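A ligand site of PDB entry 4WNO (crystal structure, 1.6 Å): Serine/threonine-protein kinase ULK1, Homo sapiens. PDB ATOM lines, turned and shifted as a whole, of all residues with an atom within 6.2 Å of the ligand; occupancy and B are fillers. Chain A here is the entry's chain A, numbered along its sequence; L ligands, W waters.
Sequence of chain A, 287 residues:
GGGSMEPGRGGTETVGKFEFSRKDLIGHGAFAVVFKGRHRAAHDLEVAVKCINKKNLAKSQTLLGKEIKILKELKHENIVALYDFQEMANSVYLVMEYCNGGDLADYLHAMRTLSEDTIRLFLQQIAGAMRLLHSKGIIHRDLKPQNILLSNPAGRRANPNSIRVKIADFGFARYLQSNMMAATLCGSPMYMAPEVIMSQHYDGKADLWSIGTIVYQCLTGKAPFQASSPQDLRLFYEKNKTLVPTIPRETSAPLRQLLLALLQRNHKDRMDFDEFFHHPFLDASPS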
ATOM      1  N   ILE A  26     -15.137 -21.972  25.698  1.00  0.00           N
ATOM      2  CA  ILE A  26     -14.595 -21.698  24.380  1.00  0.00           C
ATOM      3  C   ILE A  26     -14.230 -23.004  23.697  1.00  0.00           C
ATOM      4  O   ILE A  26     -14.494 -23.201  22.513  1.00  0.00           O
ATOM      5  CB  ILE A  26     -13.371 -20.777  24.473  1.00  0.00           C
ATOM      6  CG1 ILE A  26     -13.799 -19.386  24.923  1.00  0.00           C
ATOM      7  CG2 ILE A  26     -12.629 -20.714  23.135  1.00  0.00           C
ATOM      8  CD1 ILE A  26     -12.691 -18.407  24.969  1.00  0.00           C
ATOM      9  N   GLY A  27     -13.624 -23.896  24.465  1.00  0.00           N
ATOM     10  CA  GLY A  27     -13.221 -25.176  23.929  1.00  0.00           C
ATOM     11  C   GLY A  27     -12.893 -26.177  25.018  1.00  0.00           C
ATOM     12  O   GLY A  27     -12.378 -25.825  26.083  1.00  0.00           O
ATOM     13  N   HIS A  28     -13.219 -27.430  24.743  1.00  0.00           N
ATOM     14  CA  HIS A  28     -12.923 -28.531  25.647  1.00  0.00           C
ATOM     15  C   HIS A  28     -11.924 -29.459  24.971  1.00  0.00           C
ATOM     16  O   HIS A  28     -12.191 -29.962  23.874  1.00  0.00           O
ATOM     17  CB  HIS A  28     -14.197 -29.275  26.030  1.00  0.00           C
ATOM     18  CG  HIS A  28     -14.007 -30.301  27.099  1.00  0.00           C
ATOM     19  ND1 HIS A  28     -13.457 -31.535  26.836  1.00  0.00           N
ATOM     20  CD2 HIS A  28     -14.306 -30.283  28.417  1.00  0.00           C
ATOM     21  CE1 HIS A  28     -13.409 -32.232  27.959  1.00  0.00           C
ATOM     22  NE2 HIS A  28     -13.921 -31.495  28.932  1.00  0.00           N
ATOM     23  N   ALA A  32      -6.661 -29.500  28.154  1.00  0.00           N
ATOM     24  CA  ALA A  32      -6.996 -28.160  28.622  1.00  0.00           C
ATOM     25  C   ALA A  32      -8.449 -27.851  28.366  1.00  0.00           C
ATOM     26  O   ALA A  32      -9.015 -28.246  27.353  1.00  0.00           O
ATOM     27  CB  ALA A  32      -6.119 -27.118  27.948  1.00  0.00           C
ATOM     28  N   VAL A  34     -10.907 -24.433  28.084  1.00  0.00           N
ATOM     29  CA  VAL A  34     -10.723 -22.992  27.884  1.00  0.00           C
ATOM     30  C   VAL A  34     -12.031 -22.235  28.055  1.00  0.00           C
ATOM     31  O   VAL A  34     -13.014 -22.564  27.407  1.00  0.00           O
ATOM     32  CB  VAL A  34     -10.122 -22.710  26.494  1.00  0.00           C
ATOM     33  CG1 VAL A  34      -9.857 -21.214  26.311  1.00  0.00           C
ATOM     34  CG2 VAL A  34      -8.826 -23.508  26.290  1.00  0.00           C
ATOM     35  N   VAL A  47     -10.695 -12.092  27.503  1.00  0.00           N
ATOM     36  CA  VAL A  47      -9.595 -13.052  27.546  1.00  0.00           C
ATOM     37  C   VAL A  47     -10.097 -14.473  27.390  1.00  0.00           C
ATOM     38  O   VAL A  47     -11.284 -14.744  27.531  1.00  0.00           O
ATOM     39  CB  VAL A  47      -8.781 -12.971  28.879  1.00  0.00           C
ATOM     40  CG1 VAL A  47      -8.157 -11.596  29.039  1.00  0.00           C
ATOM     41  CG2 VAL A  47      -9.672 -13.302  30.075  1.00  0.00           C
ATOM     42  N   ALA A  48      -9.178 -15.384  27.074  1.00  0.00           N
ATOM     43  CA  ALA A  48      -9.448 -16.819  27.111  1.00  0.00           C
ATOM     44  C   ALA A  48      -8.595 -17.407  28.217  1.00  0.00           C
ATOM     45  O   ALA A  48      -7.381 -17.196  28.258  1.00  0.00           O
ATOM     46  CB  ALA A  48      -9.125 -17.467  25.748  1.00  0.00           C
ATOM     47  N   VAL A  49      -9.217 -18.150  29.131  1.00  0.00           N
ATOM     48  CA  VAL A  49      -8.462 -18.707  30.243  1.00  0.00           C
ATOM     49  C   VAL A  49      -8.354 -20.206  30.071  1.00  0.00           C
ATOM     50  O   VAL A  49      -9.378 -20.910  30.054  1.00  0.00           O
ATOM     51  CB  VAL A  49      -9.115 -18.378  31.616  1.00  0.00           C
ATOM     52  CG1 VAL A  49      -8.250 -18.923  32.769  1.00  0.00           C
ATOM     53  CG2 VAL A  49      -9.312 -16.850  31.750  1.00  0.00           C
ATOM     54  N   LYS A  50      -7.124 -20.696  29.915  1.00  0.00           N
ATOM     55  CA  LYS A  50      -6.866 -22.127  29.824  1.00  0.00           C
ATOM     56  C   LYS A  50      -6.696 -22.704  31.221  1.00  0.00           C
ATOM     57  O   LYS A  50      -5.986 -22.138  32.057  1.00  0.00           O
ATOM     58  CB  LYS A  50      -5.608 -22.421  28.994  1.00  0.00           C
ATOM     59  CG  LYS A  50      -5.722 -22.009  27.552  1.00  0.00           C
ATOM     60  CD  LYS A  50      -4.480 -22.372  26.734  1.00  0.00           C
ATOM     61  CE  LYS A  50      -4.391 -23.844  26.390  1.00  0.00           C
ATOM     62  NZ  LYS A  50      -3.445 -24.093  25.238  1.00  0.00           N
ATOM     63  N   VAL A  80      -0.745 -16.037  19.842  1.00  0.00           N
ATOM     64  CA  VAL A  80      -1.716 -15.680  20.865  1.00  0.00           C
ATOM     65  C   VAL A  80      -0.990 -15.295  22.141  1.00  0.00           C
ATOM     66  O   VAL A  80      -0.146 -16.032  22.635  1.00  0.00           O
ATOM     67  CB  VAL A  80      -2.720 -16.829  21.143  1.00  0.00           C
ATOM     68  CG1 VAL A  80      -3.809 -16.359  22.088  1.00  0.00           C
ATOM     69  CG2 VAL A  80      -3.352 -17.318  19.854  1.00  0.00           C
ATOM     70  N   MET A  96      -5.081 -15.620  28.436  1.00  0.00           N
ATOM     71  CA  MET A  96      -4.607 -15.363  27.077  1.00  0.00           C
ATOM     72  C   MET A  96      -5.425 -14.341  26.356  1.00  0.00           C
ATOM     73  O   MET A  96      -6.596 -14.109  26.665  1.00  0.00           O
ATOM     74  CB  MET A  96      -4.615 -16.658  26.280  1.00  0.00           C
ATOM     75  CG  MET A  96      -4.076 -17.800  27.102  1.00  0.00           C
ATOM     76  SD  MET A  96      -3.409 -19.067  26.062  1.00  0.00           S
ATOM     77  CE  MET A  96      -2.093 -18.120  25.260  1.00  0.00           C
ATOM     78  N   GLU A  97      -4.784 -13.692  25.385  1.00  0.00           N
ATOM     79  CA  GLU A  97      -5.484 -12.903  24.391  1.00  0.00           C
ATOM     80  C   GLU A  97      -6.708 -13.627  23.829  1.00  0.00           C
ATOM     81  O   GLU A  97      -6.638 -14.820  23.485  1.00  0.00           O
ATOM     82  CB  GLU A  97      -4.492 -12.566  23.273  1.00  0.00           C
ATOM     83  CG  GLU A  97      -5.096 -11.859  22.072  1.00  0.00           C
ATOM     84  CD  GLU A  97      -4.080 -11.675  20.965  1.00  0.00           C
ATOM     85  OE1 GLU A  97      -2.992 -12.295  21.046  1.00  0.00           O
ATOM     86  OE2 GLU A  97      -4.383 -10.919  20.023  1.00  0.00           O
ATOM     87  N   TYR A  98      -7.825 -12.919  23.748  1.00  0.00           N
ATOM     88  CA  TYR A  98      -9.015 -13.475  23.096  1.00  0.00           C
ATOM     89  C   TYR A  98      -8.996 -13.160  21.611  1.00  0.00           C
ATOM     90  O   TYR A  98      -8.951 -11.992  21.184  1.00  0.00           O
ATOM     91  CB  TYR A  98     -10.308 -12.942  23.723  1.00  0.00           C
ATOM     92  CG  TYR A  98     -11.552 -13.489  23.049  1.00  0.00           C
ATOM     93  CD1 TYR A  98     -11.924 -14.821  23.219  1.00  0.00           C
ATOM     94  CD2 TYR A  98     -12.325 -12.681  22.230  1.00  0.00           C
ATOM     95  CE1 TYR A  98     -13.062 -15.334  22.592  1.00  0.00           C
ATOM     96  CE2 TYR A  98     -13.454 -13.186  21.595  1.00  0.00           C
ATOM     97  CZ  TYR A  98     -13.817 -14.513  21.794  1.00  0.00           C
ATOM     98  OH  TYR A  98     -14.936 -15.015  21.173  1.00  0.00           O
ATOM     99  N   CYS A  99      -9.064 -14.227  20.833  1.00  0.00           N
ATOM    100  CA  CYS A  99      -9.120 -14.130  19.379  1.00  0.00           C
ATOM    101  C   CYS A  99     -10.572 -14.262  18.951  1.00  0.00           C
ATOM    102  O   CYS A  99     -11.213 -15.298  19.199  1.00  0.00           O
ATOM    103  CB  CYS A  99      -8.250 -15.215  18.729  1.00  0.00           C
ATOM    104  SG  CYS A  99      -6.514 -15.110  19.224  1.00  0.00           S
ATOM    105  N   ASN A 100     -11.108 -13.214  18.327  1.00  0.00           N
ATOM    106  CA  ASN A 100     -12.560 -13.140  18.124  1.00  0.00           C
ATOM    107  C   ASN A 100     -13.074 -13.706  16.812  1.00  0.00           C
ATOM    108  O   ASN A 100     -14.214 -13.432  16.438  1.00  0.00           O
ATOM    109  CB  ASN A 100     -13.000 -11.672  18.270  1.00  0.00           C
ATOM    110  CG  ASN A 100     -12.478 -10.771  17.153  1.00  0.00           C
ATOM    111  OD1 ASN A 100     -11.932 -11.240  16.159  1.00  0.00           O
ATOM    112  ND2 ASN A 100     -12.689  -9.463  17.303  1.00  0.00           N
ATOM    113  N   GLY A 101     -12.241 -14.483  16.111  1.00  0.00           N
ATOM    114  CA  GLY A 101     -12.581 -14.954  14.778  1.00  0.00           C
ATOM    115  C   GLY A 101     -12.705 -16.464  14.656  1.00  0.00           C
ATOM    116  O   GLY A 101     -12.919 -16.976  13.567  1.00  0.00           O
ATOM    117  N   GLY A 102     -12.584 -17.166  15.786  1.00  0.00           N
ATOM    118  CA  GLY A 102     -12.603 -18.632  15.747  1.00  0.00           C
ATOM    119  C   GLY A 102     -11.302 -19.202  15.179  1.00  0.00           C
ATOM    120  O   GLY A 102     -10.272 -18.530  15.142  1.00  0.00           O
ATOM    121  N   ASP A 103     -11.327 -20.439  14.725  1.00  0.00           N
ATOM    122  CA  ASP A 103     -10.107 -21.053  14.203  1.00  0.00           C
ATOM    123  C   ASP A 103     -10.097 -21.214  12.690  1.00  0.00           C
ATOM    124  O   ASP A 103     -11.120 -21.083  12.001  1.00  0.00           O
ATOM    125  CB  ASP A 103      -9.820 -22.413  14.878  1.00  0.00           C
ATOM    126  CG  ASP A 103     -10.819 -23.492  14.527  1.00  0.00           C
ATOM    127  OD1 ASP A 103     -11.736 -23.245  13.715  1.00  0.00           O
ATOM    128  OD2 ASP A 103     -10.679 -24.612  15.064  1.00  0.00           O
ATOM    129  N   GLN A 146      -6.582 -26.121  13.359  1.00  0.00           N
ATOM    130  CA  GLN A 146      -7.273 -25.953  14.630  1.00  0.00           C
ATOM    131  C   GLN A 146      -6.500 -25.100  15.630  1.00  0.00           C
ATOM    132  O   GLN A 146      -7.102 -24.566  16.569  1.00  0.00           O
ATOM    133  CB  GLN A 146      -7.556 -27.332  15.258  1.00  0.00           C
ATOM    134  CG  GLN A 146      -8.540 -28.187  14.472  1.00  0.00           C
ATOM    135  CD  GLN A 146      -7.908 -28.968  13.331  1.00  0.00           C
ATOM    136  OE1 GLN A 146      -6.747 -28.783  12.990  1.00  0.00           O
ATOM    137  NE2 GLN A 146      -8.706 -29.862  12.739  1.00  0.00           N
ATOM    138  N   ASN A 147      -5.189 -24.980  15.428  1.00  0.00           N
ATOM    139  CA  ASN A 147      -4.329 -24.203  16.320  1.00  0.00           C
ATOM    140  C   ASN A 147      -3.911 -22.881  15.696  1.00  0.00           C
ATOM    141  O   ASN A 147      -3.016 -22.204  16.205  1.00  0.00           O
ATOM    142  CB  ASN A 147      -3.087 -24.990  16.718  1.00  0.00           C
ATOM    143  CG  ASN A 147      -3.387 -26.023  17.760  1.00  0.00           C
ATOM    144  OD1 ASN A 147      -4.408 -25.935  18.435  1.00  0.00           O
ATOM    145  ND2 ASN A 147      -2.529 -27.038  17.885  1.00  0.00           N
ATOM    146  N   LEU A 149      -5.588 -19.358  15.108  1.00  0.00           N
ATOM    147  CA  LEU A 149      -6.791 -18.602  15.443  1.00  0.00           C
ATOM    148  C   LEU A 149      -6.889 -17.317  14.666  1.00  0.00           C
ATOM    149  O   LEU A 149      -5.877 -16.733  14.267  1.00  0.00           O
ATOM    150  CB  LEU A 149      -6.841 -18.305  16.945  1.00  0.00           C
ATOM    151  CG  LEU A 149      -6.684 -19.572  17.791  1.00  0.00           C
ATOM    152  CD1 LEU A 149      -6.921 -19.259  19.278  1.00  0.00           C
ATOM    153  CD2 LEU A 149      -7.590 -20.713  17.317  1.00  0.00           C
ATOM    154  N   LEU A 150      -8.122 -16.893  14.423  1.00  0.00           N
ATOM    155  CA  LEU A 150      -8.401 -15.667  13.686  1.00  0.00           C
ATOM    156  C   LEU A 150      -8.800 -14.558  14.646  1.00  0.00           C
ATOM    157  O   LEU A 150      -9.444 -14.812  15.658  1.00  0.00           O
ATOM    158  CB  LEU A 150      -9.534 -15.852  12.673  1.00  0.00           C
ATOM    159  CG  LEU A 150      -9.265 -16.490  11.316  1.00  0.00           C
ATOM    160  CD1 LEU A 150      -8.688 -17.858  11.517  1.00  0.00           C
ATOM    161  CD2 LEU A 150     -10.533 -16.560  10.493  1.00  0.00           C
ATOM    162  N   ALA A 168      -1.590 -20.701  18.163  1.00  0.00           N
ATOM    163  CA  ALA A 168      -1.975 -21.084  19.517  1.00  0.00           C
ATOM    164  C   ALA A 168      -1.408 -22.440  19.916  1.00  0.00           C
ATOM    165  O   ALA A 168      -0.900 -23.190  19.064  1.00  0.00           O
ATOM    166  CB  ALA A 168      -3.491 -21.116  19.648  1.00  0.00           C
ATOM    167  N   ASP A 169      -1.535 -22.741  21.208  1.00  0.00           N
ATOM    168  CA  ASP A 169      -1.317 -24.073  21.789  1.00  0.00           C
ATOM    169  C   ASP A 169       0.125 -24.550  21.668  1.00  0.00           C
ATOM    170  O   ASP A 169       0.465 -25.422  20.853  1.00  0.00           O
ATOM    171  CB  ASP A 169      -2.297 -25.075  21.156  1.00  0.00           C
ATOM    172  CG  ASP A 169      -3.759 -24.772  21.531  1.00  0.00           C
ATOM    173  OD1 ASP A 169      -4.018 -23.893  22.388  1.00  0.00           O
ATOM    174  OD2 ASP A 169      -4.670 -25.426  20.978  1.00  0.00           O
HETATM  175  C1  LIG L   1     -13.245 -17.694  19.506  1.00  0.00           C
HETATM  176  C2  LIG L   1     -15.118 -18.728  18.337  1.00  0.00           C
HETATM  177  C3  LIG L   1     -11.353 -19.179  20.311  1.00  0.00           C
HETATM  178  C4  LIG L   1      -7.660 -18.500  22.867  1.00  0.00           C
HETATM  179  C5  LIG L   1      -5.917 -19.972  22.841  1.00  0.00           C
HETATM  180  C6  LIG L   1      -8.750 -19.092  22.217  1.00  0.00           C
HETATM  181  N1  LIG L   1      -6.700 -24.187  23.404  1.00  0.00           N
HETATM  182  C7  LIG L   1      -7.789 -23.813  22.561  1.00  0.00           C
HETATM  183  C8  LIG L   1      -9.096 -24.077  22.958  1.00  0.00           C
HETATM  184  C9  LIG L   1     -10.160 -23.719  22.124  1.00  0.00           C
HETATM  185  C10 LIG L   1      -7.520 -23.213  21.347  1.00  0.00           C
HETATM  186  C11 LIG L   1      -8.575 -22.854  20.498  1.00  0.00           C
HETATM  187  C12 LIG L   1      -9.877 -23.094  20.914  1.00  0.00           C
HETATM  188  N2  LIG L   1     -10.948 -22.754  20.038  1.00  0.00           N
HETATM  189  C13 LIG L   1     -11.471 -21.439  19.941  1.00  0.00           C
HETATM  190  N3  LIG L   1     -12.635 -21.312  19.315  1.00  0.00           N
HETATM  191  C14 LIG L   1     -13.241 -20.093  19.154  1.00  0.00           C
HETATM  192  C15 LIG L   1     -12.619 -18.961  19.650  1.00  0.00           C
HETATM  193  C16 LIG L   1     -14.489 -17.580  18.846  1.00  0.00           C
HETATM  194  C17 LIG L   1     -14.524 -19.987  18.494  1.00  0.00           C
HETATM  195  N4  LIG L   1     -10.693 -18.032  20.813  1.00  0.00           N
HETATM  196  C18 LIG L   1      -9.506 -18.062  21.609  1.00  0.00           C
HETATM  197  N5  LIG L   1      -8.919 -16.882  21.889  1.00  0.00           N
HETATM  198  N6  LIG L   1      -7.829 -17.175  22.641  1.00  0.00           N
HETATM  199  C19 LIG L   1      -6.407 -18.871  23.759  1.00  0.00           C
HETATM  200  C20 LIG L   1      -6.813 -20.328  24.002  1.00  0.00           C
HETATM  201  N7  LIG L   1     -10.808 -20.400  20.444  1.00  0.00           N
HETATM  202  O   HOH W   1     -13.054 -24.720  20.300  1.00  0.00           O
HETATM  203  O   HOH W   2     -13.303 -23.372  17.491  1.00  0.00           O
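A nitrogen (N6) of the ligand is in hydrogen-bond range of the backbone carbonyl oxygen of Glu 97 (2.8 Å).
N5 of the ligand is in hydrogen-bond range of N of Cys 99.
O of Cys 99 lies close to N4 of the ligand (3.2 Å).
The side-chain carboxylate of Asp 169 is in hydrogen-bond range of a nitrogen (N1) of the ligand (2.9 Å).
The side-chain amino group (NZ) of Lys 50 is in salt-bridge range of the side-chain carboxylate (OD1) of Asp 169 (2.9 Å).
The side-chain amide oxygen (OD1) of Asn 147 sits close to the side-chain carboxylate (OD2) of Asp 169, 2.6 Å away.
N of Ile 26 is in hydrogen-bond range of O of Val 34.
The backbone carbonyl oxygen (O) of Ala 48 sits at hydrogen-bond distance from the backbone NH (N) of Met 96, at 2.8 Å.
N of Val 34 lies within hydrogen-bond range of O of Gly 27.
The backbone NH (N) of Leu 150 is in hydrogen-bond range of the backbone carbonyl oxygen (O) of Gly 102 (2.8 Å).
Residues that only touch the ligand: Ile 26 (3.3 Å), Ala 48 (3.4 Å), Val 34 (3.4 Å), Leu 149 (3.5 Å), Tyr 98 (3.5 Å), Gly 102 (3.6 Å), Lys 50 (3.7 Å), Met 96 (3.8 Å), Gly 27 (3.8 Å) and Val 80 (3.98 Å).
Hydrophobic or aromatic side chains that line the ligand: Ile 26, Val 34, Ala 48, Val 80, Met 96, Tyr 98 and Leu 149.
13 residues have an atom within 4 Å of the ligand: Ile 26, Gly 27, Val 34, Ala 48, Lys 50, Val 80, Met 96, Glu 97, Tyr 98, Cys 99, Gly 102, Leu 149 and Asp 169.
Along chain A the residues within 4 Å of the ligand span positions 26 to 169.
Water W1 lies within hydrogen-bond range of a nitrogen (N2) of the ligand and the backbone carbonyl oxygen (O) of Ile 26.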
